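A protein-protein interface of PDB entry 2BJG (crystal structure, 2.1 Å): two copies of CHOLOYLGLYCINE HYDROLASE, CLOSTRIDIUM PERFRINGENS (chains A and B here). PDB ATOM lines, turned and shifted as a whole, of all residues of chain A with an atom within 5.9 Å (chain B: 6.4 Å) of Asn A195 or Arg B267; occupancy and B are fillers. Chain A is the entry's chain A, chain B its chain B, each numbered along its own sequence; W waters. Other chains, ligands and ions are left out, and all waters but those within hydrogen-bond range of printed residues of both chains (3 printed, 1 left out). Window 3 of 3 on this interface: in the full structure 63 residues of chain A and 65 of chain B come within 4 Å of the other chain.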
ATOM      1  N   ARG A 193      -9.988  -4.469  11.417  1.00  0.00           N
ATOM      2  CA  ARG A 193     -10.984  -5.492  11.734  1.00  0.00           C
ATOM      3  C   ARG A 193     -12.132  -4.922  12.564  1.00  0.00           C
ATOM      4  O   ARG A 193     -11.908  -4.232  13.561  1.00  0.00           O
ATOM      5  CB  ARG A 193     -10.340  -6.666  12.477  1.00  0.00           C
ATOM      6  CG  ARG A 193      -9.488  -7.578  11.610  1.00  0.00           C
ATOM      7  CD  ARG A 193      -8.806  -8.659  12.443  1.00  0.00           C
ATOM      8  NE  ARG A 193      -7.645  -8.153  13.184  1.00  0.00           N
ATOM      9  CZ  ARG A 193      -6.862  -8.895  13.967  1.00  0.00           C
ATOM     10  NH1 ARG A 193      -7.107 -10.190  14.128  1.00  0.00           N
ATOM     11  NH2 ARG A 193      -5.833  -8.334  14.599  1.00  0.00           N
ATOM     12  N   TYR A 194     -13.363  -5.224  12.157  1.00  0.00           N
ATOM     13  CA  TYR A 194     -14.550  -4.767  12.886  1.00  0.00           C
ATOM     14  C   TYR A 194     -14.788  -5.595  14.147  1.00  0.00           C
ATOM     15  O   TYR A 194     -15.451  -5.135  15.079  1.00  0.00           O
ATOM     16  CB  TYR A 194     -15.798  -4.778  11.987  1.00  0.00           C
ATOM     17  CG  TYR A 194     -15.597  -4.114  10.643  1.00  0.00           C
ATOM     18  CD1 TYR A 194     -15.047  -2.832  10.551  1.00  0.00           C
ATOM     19  CD2 TYR A 194     -15.958  -4.765   9.465  1.00  0.00           C
ATOM     20  CE1 TYR A 194     -14.851  -2.220   9.321  1.00  0.00           C
ATOM     21  CE2 TYR A 194     -15.770  -4.157   8.222  1.00  0.00           C
ATOM     22  CZ  TYR A 194     -15.216  -2.887   8.162  1.00  0.00           C
ATOM     23  OH  TYR A 194     -15.027  -2.280   6.946  1.00  0.00           O
ATOM     24  N   ASN A 195     -14.235  -6.807  14.168  1.00  0.00           N
ATOM     25  CA  ASN A 195     -14.390  -7.724  15.296  1.00  0.00           C
ATOM     26  C   ASN A 195     -13.360  -7.501  16.396  1.00  0.00           C
ATOM     27  O   ASN A 195     -12.184  -7.245  16.123  1.00  0.00           O
ATOM     28  CB  ASN A 195     -14.341  -9.185  14.828  1.00  0.00           C
ATOM     29  CG  ASN A 195     -15.443  -9.521  13.836  1.00  0.00           C
ATOM     30  OD1 ASN A 195     -16.542  -8.963  13.894  1.00  0.00           O
ATOM     31  ND2 ASN A 195     -15.153 -10.444  12.922  1.00  0.00           N
ATOM     32  N   GLN A 196     -13.824  -7.610  17.638  1.00  0.00           N
ATOM     33  CA  GLN A 196     -12.991  -7.449  18.825  1.00  0.00           C
ATOM     34  C   GLN A 196     -11.837  -8.449  18.848  1.00  0.00           C
ATOM     35  O   GLN A 196     -12.025  -9.641  18.603  1.00  0.00           O
ATOM     36  CB  GLN A 196     -13.853  -7.579  20.096  1.00  0.00           C
ATOM     37  CG  GLN A 196     -13.092  -7.534  21.437  1.00  0.00           C
ATOM     38  CD  GLN A 196     -12.585  -6.148  21.814  1.00  0.00           C
ATOM     39  OE1 GLN A 196     -12.497  -5.248  20.974  1.00  0.00           O
ATOM     40  NE2 GLN A 196     -12.242  -5.971  23.088  1.00  0.00           N
ATOM     41  N   VAL A 197     -10.639  -7.933  19.110  1.00  0.00           N
ATOM     42  CA  VAL A 197      -9.469  -8.763  19.388  1.00  0.00           C
ATOM     43  C   VAL A 197      -9.287  -8.732  20.908  1.00  0.00           C
ATOM     44  O   VAL A 197      -8.848  -7.716  21.454  1.00  0.00           O
ATOM     45  CB  VAL A 197      -8.196  -8.242  18.674  1.00  0.00           C
ATOM     46  CG1 VAL A 197      -7.029  -9.208  18.881  1.00  0.00           C
ATOM     47  CG2 VAL A 197      -8.457  -8.024  17.185  1.00  0.00           C
ATOM     48  N   GLN A 212     -13.860  -2.444  24.157  1.00  0.00           N
ATOM     49  CA  GLN A 212     -14.241  -2.735  22.774  1.00  0.00           C
ATOM     50  C   GLN A 212     -13.535  -1.817  21.778  1.00  0.00           C
ATOM     51  O   GLN A 212     -13.220  -0.675  22.098  1.00  0.00           O
ATOM     52  CB  GLN A 212     -15.761  -2.607  22.597  1.00  0.00           C
ATOM     53  CG  GLN A 212     -16.583  -3.612  23.389  1.00  0.00           C
ATOM     54  CD  GLN A 212     -16.319  -5.049  22.980  1.00  0.00           C
ATOM     55  OE1 GLN A 212     -16.157  -5.353  21.798  1.00  0.00           O
ATOM     56  NE2 GLN A 212     -16.280  -5.941  23.957  1.00  0.00           N
ATOM     57  N   GLY A 213     -13.283  -2.332  20.578  1.00  0.00           N
ATOM     58  CA  GLY A 213     -12.765  -1.526  19.479  1.00  0.00           C
ATOM     59  C   GLY A 213     -11.313  -1.722  19.082  1.00  0.00           C
ATOM     60  O   GLY A 213     -10.794  -0.970  18.250  1.00  0.00           O
ATOM     61  N   THR A 214     -10.655  -2.733  19.650  1.00  0.00           N
ATOM     62  CA  THR A 214      -9.220  -2.942  19.414  1.00  0.00           C
ATOM     63  C   THR A 214      -8.840  -3.292  17.972  1.00  0.00           C
ATOM     64  O   THR A 214      -7.691  -3.083  17.569  1.00  0.00           O
ATOM     65  CB  THR A 214      -8.606  -3.994  20.375  1.00  0.00           C
ATOM     66  OG1 THR A 214      -9.315  -5.235  20.258  1.00  0.00           O
ATOM     67  CG2 THR A 214      -8.651  -3.499  21.821  1.00  0.00           C
ATOM     68  N   GLY A 215      -9.791  -3.816  17.201  1.00  0.00           N
ATOM     69  CA  GLY A 215      -9.527  -4.200  15.810  1.00  0.00           C
ATOM     70  C   GLY A 215      -9.311  -3.024  14.871  1.00  0.00           C
ATOM     71  O   GLY A 215      -8.715  -3.182  13.795  1.00  0.00           O
ATOM     72  N   ASN A 242     -22.332  -6.306   8.248  1.00  0.00           N
ATOM     73  CA  ASN A 242     -22.880  -6.831   9.495  1.00  0.00           C
ATOM     74  C   ASN A 242     -24.364  -6.541   9.744  1.00  0.00           C
ATOM     75  O   ASN A 242     -25.011  -7.281  10.478  1.00  0.00           O
ATOM     76  CB  ASN A 242     -22.036  -6.360  10.692  1.00  0.00           C
ATOM     77  CG  ASN A 242     -20.601  -6.871  10.637  1.00  0.00           C
ATOM     78  OD1 ASN A 242     -19.669  -6.190  11.073  1.00  0.00           O
ATOM     79  ND2 ASN A 242     -20.418  -8.071  10.093  1.00  0.00           N
ATOM     80  N   ASP A 243     -24.895  -5.477   9.141  1.00  0.00           N
ATOM     81  CA  ASP A 243     -26.246  -4.990   9.480  1.00  0.00           C
ATOM     82  C   ASP A 243     -27.053  -4.464   8.285  1.00  0.00           C
ATOM     83  O   ASP A 243     -27.765  -3.461   8.399  1.00  0.00           O
ATOM     84  CB  ASP A 243     -26.155  -3.912  10.566  1.00  0.00           C
ATOM     85  CG  ASP A 243     -25.694  -4.466  11.900  1.00  0.00           C
ATOM     86  OD1 ASP A 243     -26.550  -4.977  12.665  1.00  0.00           O
ATOM     87  OD2 ASP A 243     -24.472  -4.385  12.185  1.00  0.00           O
ATOM     88  N   GLY B 264     -22.360  -1.712  13.365  1.00  0.00           N
ATOM     89  CA  GLY B 264     -21.616  -2.545  12.433  1.00  0.00           C
ATOM     90  C   GLY B 264     -20.113  -2.598  12.622  1.00  0.00           C
ATOM     91  O   GLY B 264     -19.491  -3.610  12.286  1.00  0.00           O
ATOM     92  N   SER B 265     -19.529  -1.524  13.162  1.00  0.00           N
ATOM     93  CA  SER B 265     -18.070  -1.365  13.169  1.00  0.00           C
ATOM     94  C   SER B 265     -17.348  -1.700  14.475  1.00  0.00           C
ATOM     95  O   SER B 265     -16.128  -1.882  14.471  1.00  0.00           O
ATOM     96  CB  SER B 265     -17.665   0.026  12.648  1.00  0.00           C
ATOM     97  OG  SER B 265     -18.457   1.049  13.217  1.00  0.00           O
ATOM     98  N   THR B 266     -18.090  -1.763  15.580  1.00  0.00           N
ATOM     99  CA  THR B 266     -17.556  -2.201  16.880  1.00  0.00           C
ATOM    100  C   THR B 266     -18.271  -3.478  17.336  1.00  0.00           C
ATOM    101  O   THR B 266     -19.231  -3.421  18.099  1.00  0.00           O
ATOM    102  CB  THR B 266     -17.695  -1.098  17.968  1.00  0.00           C
ATOM    103  OG1 THR B 266     -17.123   0.128  17.498  1.00  0.00           O
ATOM    104  CG2 THR B 266     -16.986  -1.504  19.254  1.00  0.00           C
ATOM    105  N   ARG B 267     -17.801  -4.627  16.852  1.00  0.00           N
ATOM    106  CA  ARG B 267     -18.442  -5.914  17.132  1.00  0.00           C
ATOM    107  C   ARG B 267     -17.810  -6.613  18.343  1.00  0.00           C
ATOM    108  O   ARG B 267     -16.586  -6.670  18.460  1.00  0.00           O
ATOM    109  CB  ARG B 267     -18.366  -6.828  15.902  1.00  0.00           C
ATOM    110  CG  ARG B 267     -18.866  -6.205  14.594  1.00  0.00           C
ATOM    111  CD  ARG B 267     -20.371  -6.329  14.441  1.00  0.00           C
ATOM    112  NE  ARG B 267     -20.775  -7.689  14.083  1.00  0.00           N
ATOM    113  CZ  ARG B 267     -22.038  -8.088  13.954  1.00  0.00           C
ATOM    114  NH1 ARG B 267     -23.039  -7.237  14.158  1.00  0.00           N
ATOM    115  NH2 ARG B 267     -22.301  -9.343  13.621  1.00  0.00           N
ATOM    116  N   THR B 268     -18.648  -7.133  19.238  1.00  0.00           N
ATOM    117  CA  THR B 268     -18.180  -7.916  20.388  1.00  0.00           C
ATOM    118  C   THR B 268     -17.810  -9.341  19.943  1.00  0.00           C
ATOM    119  O   THR B 268     -18.037  -9.713  18.783  1.00  0.00           O
ATOM    120  CB  THR B 268     -19.251  -7.986  21.514  1.00  0.00           C
ATOM    121  OG1 THR B 268     -20.399  -8.704  21.049  1.00  0.00           O
ATOM    122  CG2 THR B 268     -19.687  -6.586  21.965  1.00  0.00           C
ATOM    123  N   VAL B 269     -17.244 -10.133  20.855  1.00  0.00           N
ATOM    124  CA  VAL B 269     -16.912 -11.540  20.559  1.00  0.00           C
ATOM    125  C   VAL B 269     -18.155 -12.437  20.413  1.00  0.00           C
ATOM    126  O   VAL B 269     -18.078 -13.536  19.854  1.00  0.00           O
ATOM    127  CB  VAL B 269     -15.899 -12.155  21.575  1.00  0.00           C
ATOM    128  CG1 VAL B 269     -14.530 -11.523  21.412  1.00  0.00           C
ATOM    129  CG2 VAL B 269     -16.391 -12.009  23.009  1.00  0.00           C
ATOM    130  N   GLU B 270     -19.295 -11.960  20.910  1.00  0.00           N
ATOM    131  CA  GLU B 270     -20.579 -12.626  20.697  1.00  0.00           C
ATOM    132  C   GLU B 270     -21.232 -12.140  19.403  1.00  0.00           C
ATOM    133  O   GLU B 270     -22.406 -12.427  19.148  1.00  0.00           O
ATOM    134  CB  GLU B 270     -21.525 -12.396  21.885  1.00  0.00           C
ATOM    135  CG  GLU B 270     -21.091 -13.064  23.198  1.00  0.00           C
ATOM    136  CD  GLU B 270     -20.031 -12.272  23.955  1.00  0.00           C
ATOM    137  OE1 GLU B 270     -20.059 -11.018  23.892  1.00  0.00           O
ATOM    138  OE2 GLU B 270     -19.176 -12.902  24.618  1.00  0.00           O
ATOM    139  N   GLU B 271     -20.466 -11.402  18.598  1.00  0.00           N
ATOM    140  CA  GLU B 271     -20.916 -10.867  17.295  1.00  0.00           C
ATOM    141  C   GLU B 271     -22.167  -9.980  17.361  1.00  0.00           C
ATOM    142  O   GLU B 271     -23.067 -10.079  16.521  1.00  0.00           O
ATOM    143  CB  GLU B 271     -21.083 -11.992  16.258  1.00  0.00           C
ATOM    144  CG  GLU B 271     -19.784 -12.744  15.950  1.00  0.00           C
ATOM    145  CD  GLU B 271     -19.905 -13.699  14.776  1.00  0.00           C
ATOM    146  OE1 GLU B 271     -21.040 -13.939  14.298  1.00  0.00           O
ATOM    147  OE2 GLU B 271     -18.855 -14.213  14.330  1.00  0.00           O
ATOM    148  N   LYS B 272     -22.210  -9.114  18.369  1.00  0.00           N
ATOM    149  CA  LYS B 272     -23.247  -8.092  18.469  1.00  0.00           C
ATOM    150  C   LYS B 272     -22.612  -6.717  18.272  1.00  0.00           C
ATOM    151  O   LYS B 272     -21.435  -6.516  18.607  1.00  0.00           O
ATOM    152  CB  LYS B 272     -23.963  -8.161  19.822  1.00  0.00           C
ATOM    153  CG  LYS B 272     -24.789  -9.434  20.036  1.00  0.00           C
ATOM    154  CD  LYS B 272     -25.879  -9.241  21.091  1.00  0.00           C
ATOM    155  CE  LYS B 272     -25.371  -9.507  22.518  1.00  0.00           C
ATOM    156  NZ  LYS B 272     -26.427  -9.271  23.566  1.00  0.00           N
ATOM    157  N   SER B 273     -23.385  -5.778  17.736  1.00  0.00           N
ATOM    158  CA  SER B 273     -22.893  -4.422  17.506  1.00  0.00           C
ATOM    159  C   SER B 273     -22.991  -3.573  18.764  1.00  0.00           C
ATOM    160  O   SER B 273     -24.076  -3.396  19.327  1.00  0.00           O
ATOM    161  CB  SER B 273     -23.639  -3.754  16.345  1.00  0.00           C
ATOM    162  OG  SER B 273     -23.251  -4.323  15.108  1.00  0.00           O
ATOM    163  N   ASP B 274     -21.839  -3.069  19.204  1.00  0.00           N
ATOM    164  CA  ASP B 274     -21.767  -2.120  20.314  1.00  0.00           C
ATOM    165  C   ASP B 274     -22.150  -0.731  19.791  1.00  0.00           C
ATOM    166  O   ASP B 274     -21.549  -0.234  18.833  1.00  0.00           O
ATOM    167  CB  ASP B 274     -20.352  -2.124  20.904  1.00  0.00           C
ATOM    168  CG  ASP B 274     -20.290  -1.572  22.322  1.00  0.00           C
ATOM    169  OD1 ASP B 274     -21.339  -1.199  22.890  1.00  0.00           O
ATOM    170  OD2 ASP B 274     -19.171  -1.507  22.878  1.00  0.00           O
HETATM  171  O   HOH W   1     -16.396  -8.651  23.370  1.00  0.00           O
HETATM  172  O   HOH W   2     -25.851  -7.895  13.851  1.00  0.00           O
HETATM  173  O   HOH W   3     -18.966  -9.550  13.555  1.00  0.00           O
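The backbone carbonyl oxygen (O) of Gly B264 lies close to the side-chain amide oxygen (OD1) of Asn A242, at 2.9 Å.
The backbone NH (N) of Gln A196 lies within hydrogen-bond range of the backbone carbonyl oxygen (O) of Arg B267, 3.0 Å away.
O of Tyr A194 lies close to O of Ser B265, at 3.4 Å.
OG of Ser B273 is in hydrogen-bond range of OD2 of Asp A243, at 3.2 Å.
The backbone carbonyl oxygen (O) of Tyr A194 is in hydrogen-bond range of the backbone NH (N) of Arg B267.
NH1 of Arg B267 is in salt-bridge range of OD2 of Asp A243, 3.8 Å away.
O of Glu B271 is in hydrogen-bond range of NH2 of Arg B267, 3.1 Å away.
The side-chain amide oxygen of Gln A196 is in hydrogen-bond range of the side-chain hydroxyl of Thr A214, 3.3 Å away.
OG1 of Thr B268 sits close to N of Glu B270, 3.4 Å away.
O of Thr B266 sits at hydrogen-bond distance from N of Asp B274 (2.9 Å).
OG1 of Thr B268 is in hydrogen-bond range of N of Lys B272 (3.3 Å).
The side-chain hydroxyl (OG) of Ser B273 lies within hydrogen-bond range of the backbone NH (N) of Gly B264.
Among the printed residues, merely in contact across the chains: Gln A212 with Asp B274 (3.4 Å), Asp A243 with Gly B264 (3.4 Å), Asn A242 with Arg B267 (3.4 Å), Asn A195 with Arg B267 (3.5 Å), Gln A212 with Thr B268 (3.6 Å), Gln A212 with Arg B267 (3.6 Å), Gln A212 with Thr B266 (3.7 Å), Tyr A194 with Gly B264 (3.9 Å) and Tyr A194 with Thr B266 (3.97 Å).
Printed residues of chain B within 4 Å of Tyr A194: Gly B264, Ser B265, Thr B266 and Arg B267.
Asn A195 touches just one residue of chain B: Arg B267 (3.5 Å).
Of the printed residues of chain B, Gln A212 touches Thr B266 (3.7 Å), Arg B267 (3.6 Å), Thr B268 (3.6 Å) and Asp B274 (3.4 Å).
Gly A215 touches none of the printed residues of chain B.
Of chain A, only Tyr A194 (3.0 Å), Asn A195 (3.5 Å), Gln A196 (3.0 Å), Gln A212 (3.6 Å), Asn A242 (3.4 Å) and Asp A243 (3.8 Å) come within 4 Å of Arg B267.
Printed residues of chain A within 4 Å of Thr B268: Gln A212 (3.6 Å).
Printed residues of chain A within 4 Å of Asp B274: Gln A212.
The nearest residue of chain B that does not touch Asn A195 is Thr B268 (5.2 Å).
Of the 11 printed residues of chain A, 6 touch a printed residue of chain B.
Along chain A the printed residues that touch a printed residue of chain B span positions 194 to 243.
Among the printed residues, 15 pairs touch across the chains.
No position is printed for both chains.
Of the 15 pairs that touch across the chains among the printed residues, none has its exchanged pair printed and touching as well.
Water W3 lies within hydrogen-bond range of the side-chain amide oxygen (OD1) of Asn A195 and the guanidinium group (NE) of Arg B267.
Water W1 lies within hydrogen-bond range of the side-chain amide nitrogen (NE2) of Gln A212 (2.8 Å) and the backbone NH (N) of Val B269 (3.0 Å).
Water W2 lies within hydrogen-bond range of NH1 of Arg B267 (2.9 Å) and OD1 of Asp A243 (3.2 Å).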
